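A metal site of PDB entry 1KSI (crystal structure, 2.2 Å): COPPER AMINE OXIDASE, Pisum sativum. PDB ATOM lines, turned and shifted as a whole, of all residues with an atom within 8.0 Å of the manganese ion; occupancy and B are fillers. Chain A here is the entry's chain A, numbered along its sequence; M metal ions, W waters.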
ATOM      1  N   LYS A  43       1.380   3.913  39.416  1.00  0.00           N
ATOM      2  CA  LYS A  43       1.260   4.930  38.358  1.00  0.00           C
ATOM      3  C   LYS A  43       1.020   6.320  38.900  1.00  0.00           C
ATOM      4  O   LYS A  43       1.743   7.244  38.448  1.00  0.00           O
ATOM      5  CB  LYS A  43       0.231   4.452  37.328  1.00  0.00           C
ATOM      6  CG  LYS A  43       0.095   5.267  36.018  1.00  0.00           C
ATOM      7  CD  LYS A  43      -1.038   4.720  35.156  1.00  0.00           C
ATOM      8  CE  LYS A  43      -0.801   4.664  33.700  1.00  0.00           C
ATOM      9  NZ  LYS A  43      -1.661   3.691  32.975  1.00  0.00           N
ATOM     10  N   ARG A 267       0.535  13.687  26.961  1.00  0.00           N
ATOM     11  CA  ARG A 267       0.837  12.309  27.139  1.00  0.00           C
ATOM     12  C   ARG A 267       0.296  11.434  26.021  1.00  0.00           C
ATOM     13  O   ARG A 267      -0.888  11.602  25.666  1.00  0.00           O
ATOM     14  CB  ARG A 267       0.206  11.696  28.454  1.00  0.00           C
ATOM     15  CG  ARG A 267       1.056  12.230  29.609  1.00  0.00           C
ATOM     16  CD  ARG A 267       0.579  11.790  30.986  1.00  0.00           C
ATOM     17  NE  ARG A 267       0.882  10.341  31.143  1.00  0.00           N
ATOM     18  CZ  ARG A 267      -0.059   9.561  31.735  1.00  0.00           C
ATOM     19  NH1 ARG A 267      -1.213  10.096  32.185  1.00  0.00           N
ATOM     20  NH2 ARG A 267       0.220   8.270  31.850  1.00  0.00           N
ATOM     21  N   VAL A 268       1.174  10.489  25.629  1.00  0.00           N
ATOM     22  CA  VAL A 268       0.737   9.531  24.648  1.00  0.00           C
ATOM     23  C   VAL A 268       0.835   8.134  25.215  1.00  0.00           C
ATOM     24  O   VAL A 268      -0.173   7.446  25.283  1.00  0.00           O
ATOM     25  CB  VAL A 268       1.547   9.642  23.355  1.00  0.00           C
ATOM     26  CG1 VAL A 268       0.944   8.739  22.270  1.00  0.00           C
ATOM     27  CG2 VAL A 268       1.553  11.076  22.843  1.00  0.00           C
ATOM     28  N   LEU A 269       2.082   7.728  25.545  1.00  0.00           N
ATOM     29  CA  LEU A 269       2.201   6.296  25.966  1.00  0.00           C
ATOM     30  C   LEU A 269       2.768   6.232  27.408  1.00  0.00           C
ATOM     31  O   LEU A 269       3.830   6.806  27.610  1.00  0.00           O
ATOM     32  CB  LEU A 269       3.124   5.585  24.981  1.00  0.00           C
ATOM     33  CG  LEU A 269       3.340   4.100  25.032  1.00  0.00           C
ATOM     34  CD1 LEU A 269       2.092   3.268  24.797  1.00  0.00           C
ATOM     35  CD2 LEU A 269       4.368   3.706  23.979  1.00  0.00           C
ATOM     36  N   TYR A 270       2.020   5.635  28.357  1.00  0.00           N
ATOM     37  CA  TYR A 270       2.661   5.488  29.682  1.00  0.00           C
ATOM     38  C   TYR A 270       3.848   4.483  29.614  1.00  0.00           C
ATOM     39  O   TYR A 270       4.991   4.766  30.044  1.00  0.00           O
ATOM     40  CB  TYR A 270       1.626   5.069  30.716  1.00  0.00           C
ATOM     41  CG  TYR A 270       2.264   5.001  32.098  1.00  0.00           C
ATOM     42  CD1 TYR A 270       2.611   6.152  32.789  1.00  0.00           C
ATOM     43  CD2 TYR A 270       2.533   3.744  32.665  1.00  0.00           C
ATOM     44  CE1 TYR A 270       3.214   6.060  34.039  1.00  0.00           C
ATOM     45  CE2 TYR A 270       3.116   3.645  33.911  1.00  0.00           C
ATOM     46  CZ  TYR A 270       3.465   4.805  34.579  1.00  0.00           C
ATOM     47  OH  TYR A 270       4.068   4.695  35.818  1.00  0.00           O
ATOM     48  N   LYS A 271       3.605   3.309  29.020  1.00  0.00           N
ATOM     49  CA  LYS A 271       4.644   2.299  28.945  1.00  0.00           C
ATOM     50  C   LYS A 271       4.456   1.394  27.748  1.00  0.00           C
ATOM     51  O   LYS A 271       3.272   1.081  27.528  1.00  0.00           O
ATOM     52  CB  LYS A 271       4.373   1.376  30.163  1.00  0.00           C
ATOM     53  CG  LYS A 271       5.335   0.168  30.316  1.00  0.00           C
ATOM     54  CD  LYS A 271       5.239  -0.263  31.787  1.00  0.00           C
ATOM     55  CE  LYS A 271       6.224  -1.324  32.217  1.00  0.00           C
ATOM     56  NZ  LYS A 271       5.618  -2.040  33.405  1.00  0.00           N
ATOM     57  N   TYR A 444       2.786  -4.862  24.605  1.00  0.00           N
ATOM     58  CA  TYR A 444       1.982  -4.339  25.714  1.00  0.00           C
ATOM     59  C   TYR A 444       1.966  -2.821  25.438  1.00  0.00           C
ATOM     60  O   TYR A 444       3.083  -2.263  25.362  1.00  0.00           O
ATOM     61  CB  TYR A 444       2.734  -4.518  27.029  1.00  0.00           C
ATOM     62  CG  TYR A 444       2.143  -3.846  28.242  1.00  0.00           C
ATOM     63  CD1 TYR A 444       1.205  -4.534  29.018  1.00  0.00           C
ATOM     64  CD2 TYR A 444       2.462  -2.573  28.625  1.00  0.00           C
ATOM     65  CE1 TYR A 444       0.631  -3.995  30.156  1.00  0.00           C
ATOM     66  CE2 TYR A 444       1.911  -1.981  29.758  1.00  0.00           C
ATOM     67  CZ  TYR A 444       1.018  -2.716  30.514  1.00  0.00           C
ATOM     68  OH  TYR A 444       0.464  -2.136  31.655  1.00  0.00           O
ATOM     69  N   LEU A 445       0.791  -2.218  25.278  1.00  0.00           N
ATOM     70  CA  LEU A 445       0.807  -0.768  24.949  1.00  0.00           C
ATOM     71  C   LEU A 445      -0.012   0.038  25.920  1.00  0.00           C
ATOM     72  O   LEU A 445      -1.223   0.192  25.682  1.00  0.00           O
ATOM     73  CB  LEU A 445       0.413  -0.539  23.470  1.00  0.00           C
ATOM     74  CG  LEU A 445       1.328  -1.135  22.405  1.00  0.00           C
ATOM     75  CD1 LEU A 445       0.588  -1.355  21.096  1.00  0.00           C
ATOM     76  CD2 LEU A 445       2.596  -0.328  22.214  1.00  0.00           C
ATOM     77  N   ASP A 446       0.578   0.541  27.012  1.00  0.00           N
ATOM     78  CA  ASP A 446      -0.271   1.296  27.939  1.00  0.00           C
ATOM     79  C   ASP A 446      -0.426   2.734  27.463  1.00  0.00           C
ATOM     80  O   ASP A 446       0.273   3.676  27.899  1.00  0.00           O
ATOM     81  CB  ASP A 446       0.235   1.212  29.379  1.00  0.00           C
ATOM     82  CG  ASP A 446      -0.584   1.958  30.390  1.00  0.00           C
ATOM     83  OD1 ASP A 446      -1.721   2.331  30.036  1.00  0.00           O
ATOM     84  OD2 ASP A 446      -0.178   2.262  31.530  1.00  0.00           O
ATOM     85  N   PHE A 447      -1.380   2.940  26.525  1.00  0.00           N
ATOM     86  CA  PHE A 447      -1.594   4.325  26.064  1.00  0.00           C
ATOM     87  C   PHE A 447      -2.311   5.142  27.128  1.00  0.00           C
ATOM     88  O   PHE A 447      -3.236   4.549  27.660  1.00  0.00           O
ATOM     89  CB  PHE A 447      -2.615   4.318  24.914  1.00  0.00           C
ATOM     90  CG  PHE A 447      -2.103   3.881  23.570  1.00  0.00           C
ATOM     91  CD1 PHE A 447      -1.297   4.720  22.845  1.00  0.00           C
ATOM     92  CD2 PHE A 447      -2.461   2.645  23.086  1.00  0.00           C
ATOM     93  CE1 PHE A 447      -0.827   4.337  21.605  1.00  0.00           C
ATOM     94  CE2 PHE A 447      -1.999   2.274  21.860  1.00  0.00           C
ATOM     95  CZ  PHE A 447      -1.190   3.105  21.114  1.00  0.00           C
ATOM     96  N   ASP A 448      -1.941   6.357  27.357  1.00  0.00           N
ATOM     97  CA  ASP A 448      -2.703   7.254  28.218  1.00  0.00           C
ATOM     98  C   ASP A 448      -2.910   8.536  27.368  1.00  0.00           C
ATOM     99  O   ASP A 448      -2.259   9.588  27.555  1.00  0.00           O
ATOM    100  CB  ASP A 448      -1.917   7.506  29.479  1.00  0.00           C
ATOM    101  CG  ASP A 448      -2.098   6.457  30.555  1.00  0.00           C
ATOM    102  OD1 ASP A 448      -2.906   5.494  30.445  1.00  0.00           O
ATOM    103  OD2 ASP A 448      -1.404   6.627  31.572  1.00  0.00           O
ATOM    104  N   ILE A 449      -3.805   8.437  26.375  1.00  0.00           N
ATOM    105  CA  ILE A 449      -3.957   9.540  25.382  1.00  0.00           C
ATOM    106  C   ILE A 449      -4.337  10.824  26.090  1.00  0.00           C
ATOM    107  O   ILE A 449      -5.485  10.901  26.537  1.00  0.00           O
ATOM    108  CB  ILE A 449      -5.022   9.158  24.331  1.00  0.00           C
ATOM    109  CG1 ILE A 449      -4.583   7.891  23.598  1.00  0.00           C
ATOM    110  CG2 ILE A 449      -5.187  10.332  23.368  1.00  0.00           C
ATOM    111  CD1 ILE A 449      -3.201   7.946  22.985  1.00  0.00           C
ATOM    112  N   GLY A 451      -3.815  11.729  29.082  1.00  0.00           N
ATOM    113  CA  GLY A 451      -4.297  11.408  30.435  1.00  0.00           C
ATOM    114  C   GLY A 451      -4.724   9.941  30.466  1.00  0.00           C
ATOM    115  O   GLY A 451      -4.562   9.283  29.436  1.00  0.00           O
ATOM    116  N   THR A 452      -5.270   9.453  31.581  1.00  0.00           N
ATOM    117  CA  THR A 452      -5.547   8.015  31.687  1.00  0.00           C
ATOM    118  C   THR A 452      -6.954   7.563  31.363  1.00  0.00           C
ATOM    119  O   THR A 452      -7.132   6.360  31.130  1.00  0.00           O
ATOM    120  CB  THR A 452      -5.273   7.508  33.147  1.00  0.00           C
ATOM    121  OG1 THR A 452      -6.207   8.151  34.024  1.00  0.00           O
ATOM    122  CG2 THR A 452      -3.870   7.823  33.640  1.00  0.00           C
ATOM    123  N   HIS A 453      -7.973   8.447  31.434  1.00  0.00           N
ATOM    124  CA  HIS A 453      -9.332   8.013  31.091  1.00  0.00           C
ATOM    125  C   HIS A 453      -9.522   7.933  29.587  1.00  0.00           C
ATOM    126  O   HIS A 453      -9.508   8.984  28.931  1.00  0.00           O
ATOM    127  CB  HIS A 453     -10.340   9.052  31.617  1.00  0.00           C
ATOM    128  CG  HIS A 453     -10.380   8.832  33.102  1.00  0.00           C
ATOM    129  ND1 HIS A 453      -9.459   9.457  33.933  1.00  0.00           N
ATOM    130  CD2 HIS A 453     -11.169   8.062  33.878  1.00  0.00           C
ATOM    131  CE1 HIS A 453      -9.679   9.089  35.184  1.00  0.00           C
ATOM    132  NE2 HIS A 453     -10.690   8.244  35.174  1.00  0.00           N
ATOM    133  N   ASN A 454      -9.740   6.737  29.057  1.00  0.00           N
ATOM    134  CA  ASN A 454      -9.736   6.560  27.622  1.00  0.00           C
ATOM    135  C   ASN A 454     -10.784   5.527  27.275  1.00  0.00           C
ATOM    136  O   ASN A 454     -11.388   4.909  28.135  1.00  0.00           O
ATOM    137  CB  ASN A 454      -8.360   6.118  27.097  1.00  0.00           C
ATOM    138  CG  ASN A 454      -7.220   7.058  27.199  1.00  0.00           C
ATOM    139  OD1 ASN A 454      -6.085   6.666  26.872  1.00  0.00           O
ATOM    140  ND2 ASN A 454      -7.218   8.322  27.598  1.00  0.00           N
ATOM    141  N   VAL A 503      -7.800   4.581  19.907  1.00  0.00           N
ATOM    142  CA  VAL A 503      -7.845   4.781  21.355  1.00  0.00           C
ATOM    143  C   VAL A 503      -8.108   6.278  21.533  1.00  0.00           C
ATOM    144  O   VAL A 503      -7.250   7.085  21.149  1.00  0.00           O
ATOM    145  CB  VAL A 503      -6.550   4.291  22.089  1.00  0.00           C
ATOM    146  CG1 VAL A 503      -6.598   4.519  23.599  1.00  0.00           C
ATOM    147  CG2 VAL A 503      -6.346   2.789  21.821  1.00  0.00           C
ATOM    148  N   THR A 550      -7.570  -4.122  27.599  1.00  0.00           N
ATOM    149  CA  THR A 550      -7.928  -4.607  28.954  1.00  0.00           C
ATOM    150  C   THR A 550      -7.997  -3.428  29.925  1.00  0.00           C
ATOM    151  O   THR A 550      -7.439  -2.366  29.590  1.00  0.00           O
ATOM    152  CB  THR A 550      -6.912  -5.635  29.550  1.00  0.00           C
ATOM    153  OG1 THR A 550      -5.563  -5.132  29.481  1.00  0.00           O
ATOM    154  CG2 THR A 550      -6.930  -6.949  28.786  1.00  0.00           C
ATOM    155  N   ALA A 551      -8.673  -3.623  31.063  1.00  0.00           N
ATOM    156  CA  ALA A 551      -8.566  -2.541  32.064  1.00  0.00           C
ATOM    157  C   ALA A 551      -7.150  -2.567  32.629  1.00  0.00           C
ATOM    158  O   ALA A 551      -6.694  -3.710  32.843  1.00  0.00           O
ATOM    159  CB  ALA A 551      -9.566  -2.761  33.170  1.00  0.00           C
ATOM    160  N   TYR A 552      -6.429  -1.504  32.847  1.00  0.00           N
ATOM    161  CA  TYR A 552      -5.139  -1.550  33.492  1.00  0.00           C
ATOM    162  C   TYR A 552      -5.142  -2.253  34.869  1.00  0.00           C
ATOM    163  O   TYR A 552      -6.045  -2.175  35.710  1.00  0.00           O
ATOM    164  CB  TYR A 552      -4.736  -0.104  33.763  1.00  0.00           C
ATOM    165  CG  TYR A 552      -3.449   0.004  34.514  1.00  0.00           C
ATOM    166  CD1 TYR A 552      -2.240  -0.154  33.851  1.00  0.00           C
ATOM    167  CD2 TYR A 552      -3.422   0.245  35.877  1.00  0.00           C
ATOM    168  CE1 TYR A 552      -1.026  -0.062  34.515  1.00  0.00           C
ATOM    169  CE2 TYR A 552      -2.205   0.348  36.533  1.00  0.00           C
ATOM    170  CZ  TYR A 552      -1.016   0.167  35.866  1.00  0.00           C
ATOM    171  OH  TYR A 552       0.178   0.253  36.539  1.00  0.00           O
ATOM    172  N   LYS A 586     -11.732   4.756  31.221  1.00  0.00           N
ATOM    173  CA  LYS A 586     -10.882   4.256  32.283  1.00  0.00           C
ATOM    174  C   LYS A 586      -9.420   4.229  31.823  1.00  0.00           C
ATOM    175  O   LYS A 586      -9.107   4.468  30.656  1.00  0.00           O
ATOM    176  CB  LYS A 586     -11.139   2.736  32.566  1.00  0.00           C
ATOM    177  CG  LYS A 586     -12.517   2.419  33.039  1.00  0.00           C
ATOM    178  CD  LYS A 586     -12.790   0.959  33.360  1.00  0.00           C
ATOM    179  CE  LYS A 586     -12.097   0.412  34.597  1.00  0.00           C
ATOM    180  NZ  LYS A 586     -12.633  -0.941  34.978  1.00  0.00           N
ATOM    181  N   ASP A 587      -8.575   3.908  32.805  1.00  0.00           N
ATOM    182  CA  ASP A 587      -7.196   3.559  32.477  1.00  0.00           C
ATOM    183  C   ASP A 587      -7.257   2.207  31.755  1.00  0.00           C
ATOM    184  O   ASP A 587      -7.783   1.195  32.254  1.00  0.00           O
ATOM    185  CB  ASP A 587      -6.290   3.659  33.682  1.00  0.00           C
ATOM    186  CG  ASP A 587      -4.855   3.646  33.193  1.00  0.00           C
ATOM    187  OD1 ASP A 587      -4.617   3.234  32.038  1.00  0.00           O
ATOM    188  OD2 ASP A 587      -3.956   4.001  33.935  1.00  0.00           O
ATOM    189  N   ILE A 588      -6.790   2.175  30.484  1.00  0.00           N
ATOM    190  CA  ILE A 588      -6.959   0.940  29.692  1.00  0.00           C
ATOM    191  C   ILE A 588      -5.616   0.689  29.030  1.00  0.00           C
ATOM    192  O   ILE A 588      -4.774   1.611  29.049  1.00  0.00           O
ATOM    193  CB  ILE A 588      -8.042   0.979  28.612  1.00  0.00           C
ATOM    194  CG1 ILE A 588      -7.812   2.207  27.723  1.00  0.00           C
ATOM    195  CG2 ILE A 588      -9.459   0.911  29.170  1.00  0.00           C
ATOM    196  CD1 ILE A 588      -8.431   2.030  26.327  1.00  0.00           C
ATOM    197  N   VAL A 589      -5.451  -0.501  28.495  1.00  0.00           N
ATOM    198  CA  VAL A 589      -4.139  -0.895  27.933  1.00  0.00           C
ATOM    199  C   VAL A 589      -4.366  -1.650  26.618  1.00  0.00           C
ATOM    200  O   VAL A 589      -5.346  -2.417  26.628  1.00  0.00           O
ATOM    201  CB  VAL A 589      -3.419  -1.906  28.904  1.00  0.00           C
ATOM    202  CG1 VAL A 589      -2.121  -2.414  28.246  1.00  0.00           C
ATOM    203  CG2 VAL A 589      -3.203  -1.265  30.258  1.00  0.00           C
ATOM    204  N   MET A 590      -3.570  -1.447  25.587  1.00  0.00           N
ATOM    205  CA  MET A 590      -3.806  -2.239  24.376  1.00  0.00           C
ATOM    206  C   MET A 590      -2.711  -3.293  24.181  1.00  0.00           C
ATOM    207  O   MET A 590      -1.528  -3.042  24.414  1.00  0.00           O
ATOM    208  CB  MET A 590      -3.803  -1.335  23.108  1.00  0.00           C
ATOM    209  CG  MET A 590      -3.993  -2.106  21.786  1.00  0.00           C
ATOM    210  SD  MET A 590      -4.321  -1.010  20.311  1.00  0.00           S
ATOM    211  CE  MET A 590      -2.619  -0.801  19.875  1.00  0.00           C
HETATM  212 MN    MN M   1      -3.796   3.525  29.946  1.00  0.00          MN
HETATM  213  O   HOH W   1      -5.914   5.071  29.387  1.00  0.00           O
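OD2 of Asp 448 is in salt-bridge range of NH1 of Arg 267 (3.5 Å).
The backbone NH (N) of Asp 448 lies within hydrogen-bond range of the backbone carbonyl oxygen (O) of Val 268, 2.9 Å away.
OD2 of Asp 587 is in salt-bridge range of NZ of Lys 43 (2.5 Å).
The backbone NH (N) of Asp 587 sits close to the backbone carbonyl oxygen (O) of Thr 452 (3.3 Å).
O of Asp 587 is in hydrogen-bond range of N of Tyr 552, 3.1 Å away.
The side-chain amino group (NZ) of Lys 43 is in salt-bridge range of the side-chain carboxylate (OD2) of Asp 446, at 2.5 Å.
O of Asp 446 sits at hydrogen-bond distance from N of Tyr 270 (2.7 Å).
N of Asp 446 sits at hydrogen-bond distance from O of Lys 271 (2.8 Å).
Lys 43 touches the manganese ion.
Of the 25 residues printed, 6 come within 4 Å of the manganese ion.
The manganese ion is bound by OD1 of Asp 448, OD1 of Asp 587, O of Ile 588, OD1 of Asp 446, O of Phe 447 and water W1.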
